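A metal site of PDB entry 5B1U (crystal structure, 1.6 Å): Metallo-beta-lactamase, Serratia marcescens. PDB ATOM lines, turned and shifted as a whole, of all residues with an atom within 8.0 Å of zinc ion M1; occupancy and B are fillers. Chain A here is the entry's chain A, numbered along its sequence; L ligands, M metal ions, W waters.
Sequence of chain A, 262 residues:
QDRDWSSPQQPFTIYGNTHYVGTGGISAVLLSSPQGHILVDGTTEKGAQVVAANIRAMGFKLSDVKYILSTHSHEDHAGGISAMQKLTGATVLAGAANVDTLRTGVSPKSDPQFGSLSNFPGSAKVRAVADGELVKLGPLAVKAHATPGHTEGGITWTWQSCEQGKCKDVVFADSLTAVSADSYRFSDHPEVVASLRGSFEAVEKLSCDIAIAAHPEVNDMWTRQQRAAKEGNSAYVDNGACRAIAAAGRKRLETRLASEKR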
ATOM      1  N   TRP A   5      11.052  -0.905  -0.643  1.00  0.00           N
ATOM      2  CA  TRP A   5      11.364  -2.106  -1.388  1.00  0.00           C
ATOM      3  C   TRP A   5      12.388  -2.989  -0.680  1.00  0.00           C
ATOM      4  O   TRP A   5      12.486  -4.180  -0.970  1.00  0.00           O
ATOM      5  CB  TRP A   5      11.992  -1.797  -2.746  1.00  0.00           C
ATOM      6  CG  TRP A   5      11.145  -1.207  -3.773  1.00  0.00           C
ATOM      7  CD1 TRP A   5       9.815  -1.136  -3.771  1.00  0.00           C
ATOM      8  CD2 TRP A   5      11.588  -0.668  -5.049  1.00  0.00           C
ATOM      9  NE1 TRP A   5       9.374  -0.534  -4.926  1.00  0.00           N
ATOM     10  CE2 TRP A   5      10.443  -0.239  -5.717  1.00  0.00           C
ATOM     11  CE3 TRP A   5      12.838  -0.444  -5.634  1.00  0.00           C
ATOM     12  CZ2 TRP A   5      10.489   0.396  -6.967  1.00  0.00           C
ATOM     13  CZ3 TRP A   5      12.891   0.171  -6.889  1.00  0.00           C
ATOM     14  CH2 TRP A   5      11.721   0.517  -7.557  1.00  0.00           C
ATOM     15  N   THR A  71      10.429 -13.677 -11.649  1.00  0.00           N
ATOM     16  CA  THR A  71       9.260 -13.108 -12.383  1.00  0.00           C
ATOM     17  C   THR A  71       9.736 -12.264 -13.541  1.00  0.00           C
ATOM     18  O   THR A  71       9.511 -12.610 -14.721  1.00  0.00           O
ATOM     19  CB  THR A  71       8.328 -12.267 -11.487  1.00  0.00           C
ATOM     20  OG1 THR A  71       9.072 -11.275 -10.814  1.00  0.00           O
ATOM     21  CG2 THR A  71       7.573 -13.167 -10.512  1.00  0.00           C
ATOM     22  N   HIS A  72      10.427 -11.177 -13.254  1.00  0.00           N
ATOM     23  CA  HIS A  72      11.011 -10.396 -14.303  1.00  0.00           C
ATOM     24  C   HIS A  72      12.209  -9.592 -13.826  1.00  0.00           C
ATOM     25  O   HIS A  72      12.432  -9.393 -12.631  1.00  0.00           O
ATOM     26  CB  HIS A  72       9.977  -9.496 -14.996  1.00  0.00           C
ATOM     27  CG  HIS A  72       9.568  -8.299 -14.198  1.00  0.00           C
ATOM     28  ND1 HIS A  72       8.491  -8.313 -13.337  1.00  0.00           N
ATOM     29  CD2 HIS A  72      10.094  -7.054 -14.107  1.00  0.00           C
ATOM     30  CE1 HIS A  72       8.364  -7.130 -12.776  1.00  0.00           C
ATOM     31  NE2 HIS A  72       9.340  -6.364 -13.193  1.00  0.00           N
ATOM     32  N   SER A  73      12.933  -9.077 -14.807  1.00  0.00           N
ATOM     33  CA  SER A  73      14.310  -8.597 -14.626  1.00  0.00           C
ATOM     34  C   SER A  73      14.437  -7.078 -14.460  1.00  0.00           C
ATOM     35  O   SER A  73      14.983  -6.406 -15.296  1.00  0.00           O
ATOM     36  CB  SER A  73      15.135  -9.078 -15.832  1.00  0.00           C
ATOM     37  OG  SER A  73      14.471  -8.764 -17.053  1.00  0.00           O
ATOM     38  N   HIS A  74      13.792  -6.554 -13.397  1.00  0.00           N
ATOM     39  CA  HIS A  74      14.018  -5.172 -12.945  1.00  0.00           C
ATOM     40  C   HIS A  74      14.621  -5.157 -11.552  1.00  0.00           C
ATOM     41  O   HIS A  74      14.479  -6.126 -10.787  1.00  0.00           O
ATOM     42  CB  HIS A  74      12.719  -4.385 -12.946  1.00  0.00           C
ATOM     43  CG  HIS A  74      12.202  -4.076 -14.300  1.00  0.00           C
ATOM     44  ND1 HIS A  74      10.874  -3.859 -14.539  1.00  0.00           N
ATOM     45  CD2 HIS A  74      12.821  -4.024 -15.509  1.00  0.00           C
ATOM     46  CE1 HIS A  74      10.694  -3.605 -15.822  1.00  0.00           C
ATOM     47  NE2 HIS A  74      11.870  -3.695 -16.429  1.00  0.00           N
ATOM     48  N   GLU A  75      15.258  -4.032 -11.199  1.00  0.00           N
ATOM     49  CA  GLU A  75      15.995  -3.966  -9.933  1.00  0.00           C
ATOM     50  C   GLU A  75      15.147  -4.321  -8.721  1.00  0.00           C
ATOM     51  O   GLU A  75      15.685  -4.820  -7.715  1.00  0.00           O
ATOM     52  CB  GLU A  75      16.635  -2.590  -9.733  1.00  0.00           C
ATOM     53  CG  GLU A  75      15.608  -1.455  -9.530  1.00  0.00           C
ATOM     54  CD  GLU A  75      16.197  -0.072  -9.241  1.00  0.00           C
ATOM     55  OE1 GLU A  75      17.190   0.035  -8.490  1.00  0.00           O
ATOM     56  OE2 GLU A  75      15.590   0.929  -9.696  1.00  0.00           O
ATOM     57  N   ASP A  76      13.861  -4.002  -8.746  1.00  0.00           N
ATOM     58  CA  ASP A  76      13.068  -4.143  -7.547  1.00  0.00           C
ATOM     59  C   ASP A  76      12.715  -5.610  -7.227  1.00  0.00           C
ATOM     60  O   ASP A  76      12.510  -5.952  -6.062  1.00  0.00           O
ATOM     61  CB  ASP A  76      11.836  -3.216  -7.563  1.00  0.00           C
ATOM     62  CG  ASP A  76      10.977  -3.310  -8.798  1.00  0.00           C
ATOM     63  OD1 ASP A  76      11.462  -3.577  -9.905  1.00  0.00           O
ATOM     64  OD2 ASP A  76       9.771  -3.049  -8.644  1.00  0.00           O
ATOM     65  N   HIS A  77      12.682  -6.450  -8.275  1.00  0.00           N
ATOM     66  CA  HIS A  77      12.329  -7.883  -8.104  1.00  0.00           C
ATOM     67  C   HIS A  77      13.539  -8.791  -8.193  1.00  0.00           C
ATOM     68  O   HIS A  77      13.590  -9.861  -7.562  1.00  0.00           O
ATOM     69  CB  HIS A  77      11.316  -8.298  -9.165  1.00  0.00           C
ATOM     70  CG  HIS A  77      10.100  -7.428  -9.165  1.00  0.00           C
ATOM     71  ND1 HIS A  77       9.145  -7.464  -8.158  1.00  0.00           N
ATOM     72  CD2 HIS A  77       9.806  -6.329  -9.921  1.00  0.00           C
ATOM     73  CE1 HIS A  77       8.270  -6.493  -8.376  1.00  0.00           C
ATOM     74  NE2 HIS A  77       8.686  -5.758  -9.389  1.00  0.00           N
ATOM     75  N   ALA A  78      14.497  -8.388  -9.024  1.00  0.00           N
ATOM     76  CA  ALA A  78      15.664  -9.215  -9.407  1.00  0.00           C
ATOM     77  C   ALA A  78      16.979  -8.689  -8.848  1.00  0.00           C
ATOM     78  O   ALA A  78      18.025  -9.375  -8.940  1.00  0.00           O
ATOM     79  CB  ALA A  78      15.811  -9.316 -10.902  1.00  0.00           C
ATOM     80  N   SER A 107      18.664  -3.766 -18.491  1.00  0.00           N
ATOM     81  CA  SER A 107      17.506  -4.041 -19.332  1.00  0.00           C
ATOM     82  C   SER A 107      17.749  -3.474 -20.725  1.00  0.00           C
ATOM     83  O   SER A 107      18.334  -2.408 -20.875  1.00  0.00           O
ATOM     84  CB  SER A 107      16.249  -3.389 -18.736  1.00  0.00           C
ATOM     85  OG  SER A 107      15.799  -4.091 -17.580  1.00  0.00           O
ATOM     86  N   ASP A 111      12.562  -2.766 -23.653  1.00  0.00           N
ATOM     87  CA  ASP A 111      11.791  -2.548 -22.416  1.00  0.00           C
ATOM     88  C   ASP A 111      11.153  -1.147 -22.455  1.00  0.00           C
ATOM     89  O   ASP A 111      11.830  -0.172 -22.734  1.00  0.00           O
ATOM     90  CB  ASP A 111      12.702  -2.726 -21.208  1.00  0.00           C
ATOM     91  CG  ASP A 111      11.953  -2.754 -19.877  1.00  0.00           C
ATOM     92  OD1 ASP A 111      11.147  -1.848 -19.599  1.00  0.00           O
ATOM     93  OD2 ASP A 111      12.279  -3.657 -19.059  1.00  0.00           O
ATOM     94  N   GLN A 113      10.423   0.830 -20.271  1.00  0.00           N
ATOM     95  CA  GLN A 113      11.065   1.757 -19.339  1.00  0.00           C
ATOM     96  C   GLN A 113      12.520   2.039 -19.659  1.00  0.00           C
ATOM     97  O   GLN A 113      13.155   2.770 -18.923  1.00  0.00           O
ATOM     98  CB  GLN A 113      10.910   1.230 -17.904  1.00  0.00           C
ATOM     99  CG  GLN A 113       9.473   1.120 -17.448  1.00  0.00           C
ATOM    100  CD  GLN A 113       9.376   0.748 -15.982  1.00  0.00           C
ATOM    101  OE1 GLN A 113       9.564   1.594 -15.104  1.00  0.00           O
ATOM    102  NE2 GLN A 113       9.141  -0.522 -15.711  1.00  0.00           N
ATOM    103  N   LEU A 117      15.427   3.046 -16.236  1.00  0.00           N
ATOM    104  CA  LEU A 117      15.636   1.967 -15.297  1.00  0.00           C
ATOM    105  C   LEU A 117      17.000   2.065 -14.678  1.00  0.00           C
ATOM    106  O   LEU A 117      17.940   2.553 -15.313  1.00  0.00           O
ATOM    107  CB  LEU A 117      15.540   0.603 -15.975  1.00  0.00           C
ATOM    108  CG  LEU A 117      14.143   0.304 -16.506  1.00  0.00           C
ATOM    109  CD1 LEU A 117      14.201  -0.767 -17.592  1.00  0.00           C
ATOM    110  CD2 LEU A 117      13.247  -0.134 -15.363  1.00  0.00           C
ATOM    111  N   HIS A 150       5.173  -6.305 -19.478  1.00  0.00           N
ATOM    112  CA  HIS A 150       5.987  -5.451 -18.632  1.00  0.00           C
ATOM    113  C   HIS A 150       7.480  -5.685 -18.966  1.00  0.00           C
ATOM    114  O   HIS A 150       8.275  -4.746 -18.922  1.00  0.00           O
ATOM    115  CB  HIS A 150       5.620  -5.697 -17.157  1.00  0.00           C
ATOM    116  CG  HIS A 150       6.365  -4.858 -16.180  1.00  0.00           C
ATOM    117  ND1 HIS A 150       5.957  -3.595 -15.789  1.00  0.00           N
ATOM    118  CD2 HIS A 150       7.380  -5.198 -15.336  1.00  0.00           C
ATOM    119  CE1 HIS A 150       6.752  -3.158 -14.828  1.00  0.00           C
ATOM    120  NE2 HIS A 150       7.672  -4.084 -14.607  1.00  0.00           N
ATOM    121  N   THR A 151       7.828  -6.940 -19.227  1.00  0.00           N
ATOM    122  CA  THR A 151       9.102  -7.315 -19.845  1.00  0.00           C
ATOM    123  C   THR A 151       8.805  -8.459 -20.823  1.00  0.00           C
ATOM    124  O   THR A 151       7.788  -9.191 -20.671  1.00  0.00           O
ATOM    125  CB  THR A 151      10.158  -7.808 -18.830  1.00  0.00           C
ATOM    126  OG1 THR A 151       9.731  -9.054 -18.258  1.00  0.00           O
ATOM    127  CG2 THR A 151      10.489  -6.804 -17.721  1.00  0.00           C
ATOM    128  N   ASP A 174       3.467 -12.312 -11.766  1.00  0.00           N
ATOM    129  CA  ASP A 174       4.335 -11.266 -12.316  1.00  0.00           C
ATOM    130  C   ASP A 174       3.562  -9.977 -12.547  1.00  0.00           C
ATOM    131  O   ASP A 174       2.329  -9.971 -12.613  1.00  0.00           O
ATOM    132  CB  ASP A 174       4.950 -11.746 -13.628  1.00  0.00           C
ATOM    133  CG  ASP A 174       6.079 -10.888 -14.112  1.00  0.00           C
ATOM    134  OD1 ASP A 174       6.639 -10.127 -13.317  1.00  0.00           O
ATOM    135  OD2 ASP A 174       6.351 -10.987 -15.313  1.00  0.00           O
ATOM    136  N   SER A 175       4.290  -8.880 -12.604  1.00  0.00           N
ATOM    137  CA  SER A 175       3.714  -7.574 -12.962  1.00  0.00           C
ATOM    138  C   SER A 175       3.148  -7.581 -14.356  1.00  0.00           C
ATOM    139  O   SER A 175       3.797  -8.003 -15.299  1.00  0.00           O
ATOM    140  CB  SER A 175       4.781  -6.504 -12.917  1.00  0.00           C
ATOM    141  OG  SER A 175       4.251  -5.314 -13.465  1.00  0.00           O
ATOM    142  N   LEU A 176       1.966  -7.002 -14.488  1.00  0.00           N
ATOM    143  CA  LEU A 176       1.284  -6.854 -15.768  1.00  0.00           C
ATOM    144  C   LEU A 176       1.089  -5.404 -16.162  1.00  0.00           C
ATOM    145  O   LEU A 176       0.127  -5.071 -16.868  1.00  0.00           O
ATOM    146  CB  LEU A 176      -0.078  -7.512 -15.683  1.00  0.00           C
ATOM    147  CG  LEU A 176      -0.103  -8.965 -15.227  1.00  0.00           C
ATOM    148  CD1 LEU A 176      -1.495  -9.513 -15.111  1.00  0.00           C
ATOM    149  CD2 LEU A 176       0.783  -9.824 -16.117  1.00  0.00           C
ATOM    150  N   THR A 177       1.959  -4.521 -15.650  1.00  0.00           N
ATOM    151  CA  THR A 177       1.733  -3.083 -15.732  1.00  0.00           C
ATOM    152  C   THR A 177       2.421  -2.434 -16.944  1.00  0.00           C
ATOM    153  O   THR A 177       3.612  -2.599 -17.187  1.00  0.00           O
ATOM    154  CB  THR A 177       2.247  -2.386 -14.473  1.00  0.00           C
ATOM    155  OG1 THR A 177       3.626  -2.732 -14.267  1.00  0.00           O
ATOM    156  CG2 THR A 177       1.437  -2.807 -13.329  1.00  0.00           C
ATOM    157  N   VAL A 179       3.982   0.579 -17.933  1.00  0.00           N
ATOM    158  CA  VAL A 179       4.688   1.770 -17.437  1.00  0.00           C
ATOM    159  C   VAL A 179       5.865   2.024 -18.392  1.00  0.00           C
ATOM    160  O   VAL A 179       6.416   1.085 -18.968  1.00  0.00           O
ATOM    161  CB  VAL A 179       5.152   1.535 -15.973  1.00  0.00           C
ATOM    162  CG1 VAL A 179       5.837   0.238 -15.815  1.00  0.00           C
ATOM    163  CG2 VAL A 179       6.066   2.633 -15.455  1.00  0.00           C
ATOM    164  N   ALA A 214       3.846  -9.770  -7.270  1.00  0.00           N
ATOM    165  CA  ALA A 214       5.240  -9.308  -7.146  1.00  0.00           C
ATOM    166  C   ALA A 214       5.378  -8.053  -6.293  1.00  0.00           C
ATOM    167  O   ALA A 214       6.239  -7.954  -5.410  1.00  0.00           O
ATOM    168  CB  ALA A 214       5.859  -9.149  -8.524  1.00  0.00           C
ATOM    169  N   HIS A 215       4.477  -7.091  -6.531  1.00  0.00           N
ATOM    170  CA  HIS A 215       4.224  -5.999  -5.586  1.00  0.00           C
ATOM    171  C   HIS A 215       3.055  -6.392  -4.708  1.00  0.00           C
ATOM    172  O   HIS A 215       1.921  -6.535  -5.178  1.00  0.00           O
ATOM    173  CB  HIS A 215       3.896  -4.678  -6.339  1.00  0.00           C
ATOM    174  CG  HIS A 215       5.060  -4.072  -7.029  1.00  0.00           C
ATOM    175  ND1 HIS A 215       5.953  -3.255  -6.383  1.00  0.00           N
ATOM    176  CD2 HIS A 215       5.602  -4.310  -8.243  1.00  0.00           C
ATOM    177  CE1 HIS A 215       6.957  -2.967  -7.179  1.00  0.00           C
ATOM    178  NE2 HIS A 215       6.777  -3.614  -8.322  1.00  0.00           N
HETATM  179  O1  LIG L   1       4.551  -3.272 -11.802  1.00  0.00           O
HETATM  180  C1  LIG L   1       5.739  -3.157 -11.470  1.00  0.00           C
HETATM  181  O2  LIG L   1       6.457  -4.231 -11.242  1.00  0.00           O
HETATM  182  C2  LIG L   1       6.257  -1.815 -11.198  1.00  0.00           C
HETATM  183  N1  LIG L   1       7.379  -1.624 -10.650  1.00  0.00           N
HETATM  184  C3  LIG L   1       5.548  -0.578 -11.627  1.00  0.00           C
HETATM  185  C4  LIG L   1       6.632   0.468 -11.371  1.00  0.00           C
HETATM  186  C5  LIG L   1       7.683  -0.203 -10.448  1.00  0.00           C
HETATM  187  C6  LIG L   1       9.158   0.066 -10.726  1.00  0.00           C
HETATM  188  C7  LIG L   1       9.500   1.465 -10.277  1.00  0.00           C
HETATM  189  O3  LIG L   1      10.600   1.919 -10.505  1.00  0.00           O
HETATM  190  O4  LIG L   1       8.708   2.132  -9.475  1.00  0.00           O
HETATM  191  C8  LIG L   1       9.557  -0.070 -12.193  1.00  0.00           C
HETATM  192  O5  LIG L   1       8.868  -1.121 -12.864  1.00  0.00           O
HETATM  193  C9  LIG L   1      11.064  -0.361 -12.307  1.00  0.00           C
HETATM  194  S1  LIG L   1       3.962  -0.391 -10.770  1.00  0.00           S
HETATM  195  C10 LIG L   1       4.319  -0.540  -9.030  1.00  0.00           C
HETATM  196  C11 LIG L   1       3.116  -0.938  -8.161  1.00  0.00           C
HETATM  197  N2  LIG L   1       2.216  -1.897  -8.759  1.00  0.00           N
HETATM  198  C12 LIG L   1       1.093  -1.539  -9.371  1.00  0.00           C
HETATM  199  N3  LIG L   1       0.351  -2.427  -9.838  1.00  0.00           N
HETATM  200 ZN    ZN M   1       9.258  -4.296 -13.283  1.00  0.00          ZN
HETATM  201 ZN    ZN M   2       8.161  -3.724  -9.924  1.00  0.00          ZN
HETATM  202  O   HOH W   1       9.339  -3.534 -11.586  1.00  0.00           O
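ND1 of His 72 lies within hydrogen-bond range of OD1 of Asp 174 (2.6 Å).
ND1 of His 150 is in hydrogen-bond range of OG of Ser 175, at 3.4 Å.
ND1 of His 150 lies within hydrogen-bond range of O of Thr 177 (2.9 Å).
A ring nitrogen (NE2) of His 74 lies within hydrogen-bond range of the side-chain carboxylate (OD2) of Asp 111 (2.7 Å).
Zinc ion M1 is bound by water W1 (1.9 Å), a ring nitrogen (NE2) of His 72 (2.1 Å), a ring nitrogen (NE2) of His 150 (2.1 Å) and a ring nitrogen (ND1) of His 74 (2.1 Å).
Zinc ion M1 has four donor atoms within binding distance.
His 77 touches zinc ion M1 (CD2 to ZN, 3.97 Å).
Four residues have an atom within 4 Å of zinc ion M1: His 72, His 74, His 77 and His 150.
Along chain A the residues within 4 Å of zinc ion M1 span positions 72 to 150.
The nearest printed residue that does not touch zinc ion M1 is Asp 76 (4.1 Å).
Water W1 bridges the side-chain carboxylate of Asp 76 (2.7 Å) and an oxygen (O5) of the ligand (2.8 Å).
The side-chain amide nitrogen of Gln 113 sits at hydrogen-bond distance from an oxygen (O5) of the ligand (2.9 Å).
An oxygen (O1) of the ligand sits at hydrogen-bond distance from the side-chain hydroxyl (OG) of Ser 175, 2.7 Å away.
OG1 of Thr 177 is in hydrogen-bond range of O1 of the ligand.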
